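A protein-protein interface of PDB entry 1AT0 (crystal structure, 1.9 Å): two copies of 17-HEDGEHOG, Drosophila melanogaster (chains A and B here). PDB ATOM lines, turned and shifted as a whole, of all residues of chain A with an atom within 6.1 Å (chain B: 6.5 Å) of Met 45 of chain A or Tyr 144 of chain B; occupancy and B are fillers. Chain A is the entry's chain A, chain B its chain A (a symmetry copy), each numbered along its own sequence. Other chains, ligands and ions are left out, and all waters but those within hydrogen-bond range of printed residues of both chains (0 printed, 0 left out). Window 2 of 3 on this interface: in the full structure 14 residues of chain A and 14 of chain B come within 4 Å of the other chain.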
ATOM      1  N   LEU A  43      19.776  19.280  -9.551  1.00  0.00           N
ATOM      2  CA  LEU A  43      19.677  17.879  -9.942  1.00  0.00           C
ATOM      3  C   LEU A  43      18.504  17.198  -9.249  1.00  0.00           C
ATOM      4  O   LEU A  43      17.804  17.815  -8.445  1.00  0.00           O
ATOM      5  CB  LEU A  43      20.987  17.129  -9.629  1.00  0.00           C
ATOM      6  CG  LEU A  43      21.559  17.031  -8.205  1.00  0.00           C
ATOM      7  CD1 LEU A  43      20.874  15.936  -7.387  1.00  0.00           C
ATOM      8  CD2 LEU A  43      23.036  16.718  -8.301  1.00  0.00           C
ATOM      9  N   PHE A  44      18.259  15.948  -9.620  1.00  0.00           N
ATOM     10  CA  PHE A  44      17.208  15.144  -9.015  1.00  0.00           C
ATOM     11  C   PHE A  44      17.923  13.997  -8.308  1.00  0.00           C
ATOM     12  O   PHE A  44      18.774  13.329  -8.903  1.00  0.00           O
ATOM     13  CB  PHE A  44      16.264  14.588 -10.079  1.00  0.00           C
ATOM     14  CG  PHE A  44      15.391  15.624 -10.706  1.00  0.00           C
ATOM     15  CD1 PHE A  44      14.154  15.931 -10.153  1.00  0.00           C
ATOM     16  CD2 PHE A  44      15.813  16.318 -11.837  1.00  0.00           C
ATOM     17  CE1 PHE A  44      13.349  16.919 -10.714  1.00  0.00           C
ATOM     18  CE2 PHE A  44      15.011  17.312 -12.409  1.00  0.00           C
ATOM     19  CZ  PHE A  44      13.779  17.611 -11.845  1.00  0.00           C
ATOM     20  N   MET A  45      17.639  13.821  -7.023  1.00  0.00           N
ATOM     21  CA  MET A  45      18.253  12.751  -6.244  1.00  0.00           C
ATOM     22  C   MET A  45      17.532  11.439  -6.515  1.00  0.00           C
ATOM     23  O   MET A  45      18.059  10.360  -6.262  1.00  0.00           O
ATOM     24  CB  MET A  45      18.206  13.101  -4.764  1.00  0.00           C
ATOM     25  CG  MET A  45      19.007  14.340  -4.436  1.00  0.00           C
ATOM     26  SD  MET A  45      18.363  14.949  -2.743  1.00  0.00           S
ATOM     27  CE  MET A  45      16.837  15.878  -3.311  1.00  0.00           C
ATOM     28  N   ASP A  46      16.317  11.556  -7.032  1.00  0.00           N
ATOM     29  CA  ASP A  46      15.486  10.421  -7.390  1.00  0.00           C
ATOM     30  C   ASP A  46      14.493  10.972  -8.391  1.00  0.00           C
ATOM     31  O   ASP A  46      14.035  12.107  -8.254  1.00  0.00           O
ATOM     32  CB  ASP A  46      14.736   9.867  -6.173  1.00  0.00           C
ATOM     33  CG  ASP A  46      15.003   8.381  -5.946  1.00  0.00           C
ATOM     34  OD1 ASP A  46      14.325   7.533  -6.570  1.00  0.00           O
ATOM     35  OD2 ASP A  46      15.902   8.062  -5.141  1.00  0.00           O
ATOM     36  N   ARG A  47      14.231  10.206  -9.438  1.00  0.00           N
ATOM     37  CA  ARG A  47      13.290  10.607 -10.466  1.00  0.00           C
ATOM     38  C   ARG A  47      12.929   9.387 -11.283  1.00  0.00           C
ATOM     39  O   ARG A  47      13.586   9.062 -12.276  1.00  0.00           O
ATOM     40  CB  ARG A  47      13.867  11.687 -11.383  1.00  0.00           C
ATOM     41  CG  ARG A  47      12.816  12.253 -12.331  1.00  0.00           C
ATOM     42  CD  ARG A  47      13.382  13.245 -13.314  1.00  0.00           C
ATOM     43  NE  ARG A  47      12.322  13.854 -14.110  1.00  0.00           N
ATOM     44  CZ  ARG A  47      11.835  13.351 -15.240  1.00  0.00           C
ATOM     45  NH1 ARG A  47      12.317  12.218 -15.732  1.00  0.00           N
ATOM     46  NH2 ARG A  47      10.847  13.975 -15.864  1.00  0.00           N
ATOM     47  N   HIS A  72      11.160  11.635   4.316  1.00  0.00           N
ATOM     48  CA  HIS A  72      11.520  12.957   3.808  1.00  0.00           C
ATOM     49  C   HIS A  72      11.452  13.985   4.947  1.00  0.00           C
ATOM     50  O   HIS A  72      10.525  13.944   5.764  1.00  0.00           O
ATOM     51  CB  HIS A  72      10.567  13.361   2.673  1.00  0.00           C
ATOM     52  CG  HIS A  72      11.102  14.444   1.784  1.00  0.00           C
ATOM     53  ND1 HIS A  72      11.259  14.274   0.425  1.00  0.00           N
ATOM     54  CD2 HIS A  72      11.549  15.694   2.058  1.00  0.00           C
ATOM     55  CE1 HIS A  72      11.793  15.366  -0.096  1.00  0.00           C
ATOM     56  NE2 HIS A  72      11.975  16.240   0.875  1.00  0.00           N
ATOM     57  N   ALA A 126      12.528  13.676  -6.465  1.00  0.00           N
ATOM     58  CA  ALA A 126      13.216  14.324  -5.357  1.00  0.00           C
ATOM     59  C   ALA A 126      14.173  15.373  -5.913  1.00  0.00           C
ATOM     60  O   ALA A 126      15.327  15.068  -6.236  1.00  0.00           O
ATOM     61  CB  ALA A 126      13.979  13.286  -4.537  1.00  0.00           C
ATOM     62  N   PRO A 127      13.685  16.609  -6.118  1.00  0.00           N
ATOM     63  CA  PRO A 127      14.559  17.657  -6.650  1.00  0.00           C
ATOM     64  C   PRO A 127      15.435  18.302  -5.585  1.00  0.00           C
ATOM     65  O   PRO A 127      15.025  18.447  -4.432  1.00  0.00           O
ATOM     66  CB  PRO A 127      13.569  18.651  -7.260  1.00  0.00           C
ATOM     67  CG  PRO A 127      12.378  18.520  -6.389  1.00  0.00           C
ATOM     68  CD  PRO A 127      12.279  17.047  -6.087  1.00  0.00           C
ATOM     69  N   LEU A 128      16.668  18.621  -5.964  1.00  0.00           N
ATOM     70  CA  LEU A 128      17.611  19.267  -5.062  1.00  0.00           C
ATOM     71  C   LEU A 128      17.905  20.663  -5.592  1.00  0.00           C
ATOM     72  O   LEU A 128      18.357  20.816  -6.730  1.00  0.00           O
ATOM     73  CB  LEU A 128      18.911  18.463  -4.975  1.00  0.00           C
ATOM     74  CG  LEU A 128      20.016  19.063  -4.106  1.00  0.00           C
ATOM     75  CD1 LEU A 128      19.569  19.113  -2.654  1.00  0.00           C
ATOM     76  CD2 LEU A 128      21.296  18.244  -4.248  1.00  0.00           C
ATOM     77  N   THR A 129      17.639  21.677  -4.776  1.00  0.00           N
ATOM     78  CA  THR A 129      17.882  23.070  -5.158  1.00  0.00           C
ATOM     79  C   THR A 129      19.195  23.552  -4.524  1.00  0.00           C
ATOM     80  O   THR A 129      19.746  22.869  -3.653  1.00  0.00           O
ATOM     81  CB  THR A 129      16.740  23.969  -4.646  1.00  0.00           C
ATOM     82  OG1 THR A 129      16.705  23.921  -3.212  1.00  0.00           O
ATOM     83  CG2 THR A 129      15.398  23.499  -5.193  1.00  0.00           C
ATOM     84  N   CYS A 143      15.015  19.233   0.944  1.00  0.00           N
ATOM     85  CA  CYS A 143      15.157  18.464  -0.288  1.00  0.00           C
ATOM     86  C   CYS A 143      15.555  17.035   0.077  1.00  0.00           C
ATOM     87  O   CYS A 143      15.350  16.106  -0.705  1.00  0.00           O
ATOM     88  CB  CYS A 143      16.238  19.067  -1.180  1.00  0.00           C
ATOM     89  SG  CYS A 143      15.753  20.578  -1.996  1.00  0.00           S
ATOM     90  N   TYR A 144      16.107  16.869   1.278  1.00  0.00           N
ATOM     91  CA  TYR A 144      16.569  15.568   1.759  1.00  0.00           C
ATOM     92  C   TYR A 144      15.455  14.596   2.135  1.00  0.00           C
ATOM     93  O   TYR A 144      14.457  14.974   2.748  1.00  0.00           O
ATOM     94  CB  TYR A 144      17.518  15.751   2.952  1.00  0.00           C
ATOM     95  CG  TYR A 144      17.941  14.448   3.606  1.00  0.00           C
ATOM     96  CD1 TYR A 144      18.843  13.585   2.975  1.00  0.00           C
ATOM     97  CD2 TYR A 144      17.424  14.066   4.851  1.00  0.00           C
ATOM     98  CE1 TYR A 144      19.220  12.372   3.566  1.00  0.00           C
ATOM     99  CE2 TYR A 144      17.793  12.856   5.449  1.00  0.00           C
ATOM    100  CZ  TYR A 144      18.690  12.017   4.802  1.00  0.00           C
ATOM    101  OH  TYR A 144      19.069  10.832   5.390  1.00  0.00           O
ATOM    102  N   ALA A 145      15.652  13.333   1.782  1.00  0.00           N
ATOM    103  CA  ALA A 145      14.693  12.285   2.086  1.00  0.00           C
ATOM    104  C   ALA A 145      15.453  11.013   2.457  1.00  0.00           C
ATOM    105  O   ALA A 145      16.694  11.004   2.328  1.00  0.00           O
ATOM    106  CB  ALA A 145      13.785  12.032   0.882  1.00  0.00           C
ATOM    107  OXT ALA A 145      14.797  10.027   2.847  1.00  0.00           O
ATOM    108  N   CYS B   1      30.009  11.202   1.493  1.00  0.00           N
ATOM    109  CA  CYS B   1      30.540  11.188   2.883  1.00  0.00           C
ATOM    110  C   CYS B   1      31.988  11.646   2.922  1.00  0.00           C
ATOM    111  O   CYS B   1      32.641  11.755   1.876  1.00  0.00           O
ATOM    112  CB  CYS B   1      30.446   9.777   3.463  1.00  0.00           C
ATOM    113  SG  CYS B   1      28.793   9.080   3.389  1.00  0.00           S
ATOM    114  N   MET B  45      23.454  11.870   7.677  1.00  0.00           N
ATOM    115  CA  MET B  45      22.815  11.046   6.657  1.00  0.00           C
ATOM    116  C   MET B  45      23.499   9.689   6.589  1.00  0.00           C
ATOM    117  O   MET B  45      22.945   8.722   6.075  1.00  0.00           O
ATOM    118  CB  MET B  45      22.876  11.754   5.312  1.00  0.00           C
ATOM    119  CG  MET B  45      22.110  13.057   5.308  1.00  0.00           C
ATOM    120  SD  MET B  45      22.775  14.053   3.819  1.00  0.00           S
ATOM    121  CE  MET B  45      24.324  14.769   4.597  1.00  0.00           C
ATOM    122  N   ALA B  71      30.665  10.011  -5.152  1.00  0.00           N
ATOM    123  CA  ALA B  71      29.365  10.605  -5.426  1.00  0.00           C
ATOM    124  C   ALA B  71      28.964  11.811  -4.571  1.00  0.00           C
ATOM    125  O   ALA B  71      27.807  12.207  -4.572  1.00  0.00           O
ATOM    126  CB  ALA B  71      28.295   9.527  -5.364  1.00  0.00           C
ATOM    127  N   HIS B  72      29.911  12.422  -3.870  1.00  0.00           N
ATOM    128  CA  HIS B  72      29.584  13.584  -3.045  1.00  0.00           C
ATOM    129  C   HIS B  72      29.684  14.862  -3.891  1.00  0.00           C
ATOM    130  O   HIS B  72      30.612  15.002  -4.695  1.00  0.00           O
ATOM    131  CB  HIS B  72      30.544  13.665  -1.848  1.00  0.00           C
ATOM    132  CG  HIS B  72      30.035  14.504  -0.715  1.00  0.00           C
ATOM    133  ND1 HIS B  72      29.869  14.003   0.559  1.00  0.00           N
ATOM    134  CD2 HIS B  72      29.623  15.795  -0.665  1.00  0.00           C
ATOM    135  CE1 HIS B  72      29.363  14.944   1.339  1.00  0.00           C
ATOM    136  NE2 HIS B  72      29.208  16.038   0.619  1.00  0.00           N
ATOM    137  N   LEU B  73      28.721  15.773  -3.735  1.00  0.00           N
ATOM    138  CA  LEU B  73      28.736  17.038  -4.478  1.00  0.00           C
ATOM    139  C   LEU B  73      29.700  18.029  -3.847  1.00  0.00           C
ATOM    140  O   LEU B  73      29.701  18.226  -2.627  1.00  0.00           O
ATOM    141  CB  LEU B  73      27.354  17.682  -4.535  1.00  0.00           C
ATOM    142  CG  LEU B  73      26.354  17.180  -5.565  1.00  0.00           C
ATOM    143  CD1 LEU B  73      25.055  17.925  -5.344  1.00  0.00           C
ATOM    144  CD2 LEU B  73      26.883  17.406  -6.978  1.00  0.00           C
ATOM    145  N   VAL B  74      30.479  18.691  -4.693  1.00  0.00           N
ATOM    146  CA  VAL B  74      31.463  19.662  -4.247  1.00  0.00           C
ATOM    147  C   VAL B  74      31.333  20.937  -5.079  1.00  0.00           C
ATOM    148  O   VAL B  74      31.011  20.870  -6.267  1.00  0.00           O
ATOM    149  CB  VAL B  74      32.890  19.055  -4.369  1.00  0.00           C
ATOM    150  CG1 VAL B  74      33.959  20.112  -4.115  1.00  0.00           C
ATOM    151  CG2 VAL B  74      33.038  17.877  -3.387  1.00  0.00           C
ATOM    152  N   PHE B  88      30.207  16.317  -8.964  1.00  0.00           N
ATOM    153  CA  PHE B  88      30.516  15.147  -8.155  1.00  0.00           C
ATOM    154  C   PHE B  88      32.026  15.087  -7.966  1.00  0.00           C
ATOM    155  O   PHE B  88      32.787  15.450  -8.869  1.00  0.00           O
ATOM    156  CB  PHE B  88      29.982  13.870  -8.806  1.00  0.00           C
ATOM    157  CG  PHE B  88      28.500  13.700  -8.658  1.00  0.00           C
ATOM    158  CD1 PHE B  88      27.945  13.418  -7.417  1.00  0.00           C
ATOM    159  CD2 PHE B  88      27.658  13.845  -9.749  1.00  0.00           C
ATOM    160  CE1 PHE B  88      26.573  13.285  -7.263  1.00  0.00           C
ATOM    161  CE2 PHE B  88      26.284  13.715  -9.607  1.00  0.00           C
ATOM    162  CZ  PHE B  88      25.740  13.435  -8.359  1.00  0.00           C
ATOM    163  N   PRO B 127      27.484  14.688   7.487  1.00  0.00           N
ATOM    164  CA  PRO B 127      26.637  15.593   8.267  1.00  0.00           C
ATOM    165  C   PRO B 127      25.782  16.508   7.401  1.00  0.00           C
ATOM    166  O   PRO B 127      26.200  16.926   6.320  1.00  0.00           O
ATOM    167  CB  PRO B 127      27.651  16.375   9.103  1.00  0.00           C
ATOM    168  CG  PRO B 127      28.842  16.435   8.223  1.00  0.00           C
ATOM    169  CD  PRO B 127      28.902  15.083   7.561  1.00  0.00           C
ATOM    170  N   LEU B 128      24.557  16.754   7.852  1.00  0.00           N
ATOM    171  CA  LEU B 128      23.635  17.630   7.143  1.00  0.00           C
ATOM    172  C   LEU B 128      23.376  18.856   8.008  1.00  0.00           C
ATOM    173  O   LEU B 128      22.925  18.731   9.149  1.00  0.00           O
ATOM    174  CB  LEU B 128      22.314  16.909   6.862  1.00  0.00           C
ATOM    175  CG  LEU B 128      21.228  17.737   6.176  1.00  0.00           C
ATOM    176  CD1 LEU B 128      21.682  18.137   4.781  1.00  0.00           C
ATOM    177  CD2 LEU B 128      19.927  16.943   6.112  1.00  0.00           C
ATOM    178  N   GLY B 132      22.668  23.232   4.252  1.00  0.00           N
ATOM    179  CA  GLY B 132      22.745  22.197   3.238  1.00  0.00           C
ATOM    180  C   GLY B 132      24.146  22.045   2.681  1.00  0.00           C
ATOM    181  O   GLY B 132      24.401  21.191   1.831  1.00  0.00           O
ATOM    182  N   ALA B 141      31.762  22.326   0.369  1.00  0.00           N
ATOM    183  CA  ALA B 141      31.105  21.195  -0.265  1.00  0.00           C
ATOM    184  C   ALA B 141      29.627  21.185   0.076  1.00  0.00           C
ATOM    185  O   ALA B 141      29.177  21.904   0.967  1.00  0.00           O
ATOM    186  CB  ALA B 141      31.748  19.894   0.207  1.00  0.00           C
ATOM    187  N   SER B 142      28.863  20.408  -0.677  1.00  0.00           N
ATOM    188  CA  SER B 142      27.443  20.263  -0.411  1.00  0.00           C
ATOM    189  C   SER B 142      27.397  19.181   0.661  1.00  0.00           C
ATOM    190  O   SER B 142      28.410  18.523   0.933  1.00  0.00           O
ATOM    191  CB  SER B 142      26.724  19.756  -1.665  1.00  0.00           C
ATOM    192  OG  SER B 142      25.392  19.362  -1.381  1.00  0.00           O
ATOM    193  N   CYS B 143      26.250  19.033   1.313  1.00  0.00           N
ATOM    194  CA  CYS B 143      26.083  17.984   2.313  1.00  0.00           C
ATOM    195  C   CYS B 143      25.648  16.703   1.602  1.00  0.00           C
ATOM    196  O   CYS B 143      25.825  15.603   2.126  1.00  0.00           O
ATOM    197  CB  CYS B 143      25.015  18.373   3.330  1.00  0.00           C
ATOM    198  SG  CYS B 143      25.538  19.618   4.498  1.00  0.00           S
ATOM    199  N   TYR B 144      25.095  16.858   0.400  1.00  0.00           N
ATOM    200  CA  TYR B 144      24.601  15.732  -0.390  1.00  0.00           C
ATOM    201  C   TYR B 144      25.689  14.856  -1.001  1.00  0.00           C
ATOM    202  O   TYR B 144      26.699  15.349  -1.503  1.00  0.00           O
ATOM    203  CB  TYR B 144      23.661  16.234  -1.496  1.00  0.00           C
ATOM    204  CG  TYR B 144      23.206  15.148  -2.454  1.00  0.00           C
ATOM    205  CD1 TYR B 144      22.278  14.179  -2.056  1.00  0.00           C
ATOM    206  CD2 TYR B 144      23.716  15.076  -3.757  1.00  0.00           C
ATOM    207  CE1 TYR B 144      21.871  13.164  -2.931  1.00  0.00           C
ATOM    208  CE2 TYR B 144      23.317  14.066  -4.638  1.00  0.00           C
ATOM    209  CZ  TYR B 144      22.396  13.116  -4.219  1.00  0.00           C
ATOM    210  OH  TYR B 144      21.987  12.126  -5.084  1.00  0.00           O
ATOM    211  N   ALA B 145      25.457  13.551  -0.976  1.00  0.00           N
ATOM    212  CA  ALA B 145      26.389  12.588  -1.536  1.00  0.00           C
ATOM    213  C   ALA B 145      25.597  11.469  -2.211  1.00  0.00           C
ATOM    214  O   ALA B 145      24.355  11.461  -2.084  1.00  0.00           O
ATOM    215  CB  ALA B 145      27.286  12.016  -0.436  1.00  0.00           C
ATOM    216  OXT ALA B 145      26.228  10.595  -2.838  1.00  0.00           O
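Of the 15 printed residues of chain B, 3 touch a printed residue of chain A.
Hydrophobic or aromatic side chains of chain B within 4 Å of the printed part of chain A: Met 45, Leu 73 and Tyr 144.
Along chain B the printed residues that touch a printed residue of chain A span positions 45 to 144.
Among the printed residues, no Asp or Glu carboxylate lies within 4 Å of a Lys or Arg side-chain nitrogen of the other chain.
The backbone carbonyl oxygen (O) of Leu 43 of chain A lies within hydrogen-bond range of the backbone NH (N) of Leu 128 of chain A, at 2.8 Å.
The backbone carbonyl oxygen (O) of Ala 126 of chain A lies within hydrogen-bond range of the backbone NH (N) of Met 45 of chain A, 2.7 Å away.
The backbone carbonyl oxygen of Tyr 144 of chain A sits close to a ring nitrogen (NE2) of His 72 of chain A (3.4 Å).
NE2 of His 72 of chain B lies close to O of Tyr 144 of chain B (3.4 Å).
O of Tyr 144 of chain B is in hydrogen-bond range of N of Leu 73 of chain B (3.0 Å).
N of Tyr 144 of chain B sits at hydrogen-bond distance from OG of Ser 142 of chain B.
Of the printed residues of chain A, Tyr 144 of chain B touches Met 45 (3.4 Å).
Of the printed residues of chain B, Leu 128 of chain A touches Leu 73 (3.9 Å).
Of the printed residues of chain B, Leu 43 of chain A touches Leu 73 (3.8 Å).
Of the printed residues of chain A, Met 45 of chain B touches Tyr 144.
Printed residues of chain A within 4 Å of Leu 73 of chain B: Leu 43 and Leu 128.
Met 45 of chain A touches Tyr 144 of chain B, and with the chains exchanged Tyr 144 of chain A touches Met 45 of chain B.
Positions printed for both chains: 45, 72, 127, 128, 143, 144 and 145.
Of the 4 pairs that touch across the chains among the printed residues, 2 have their exchanged pair printed and touching as well.
Among the printed residues, pairs that only touch across the chains: Met 45 of chain A with Tyr 144 of chain B (3.4 Å), Tyr 144 of chain A with Met 45 of chain B (3.4 Å), Leu 43 of chain A with Leu 73 of chain B (3.8 Å) and Leu 128 of chain A with Leu 73 of chain B (3.9 Å).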
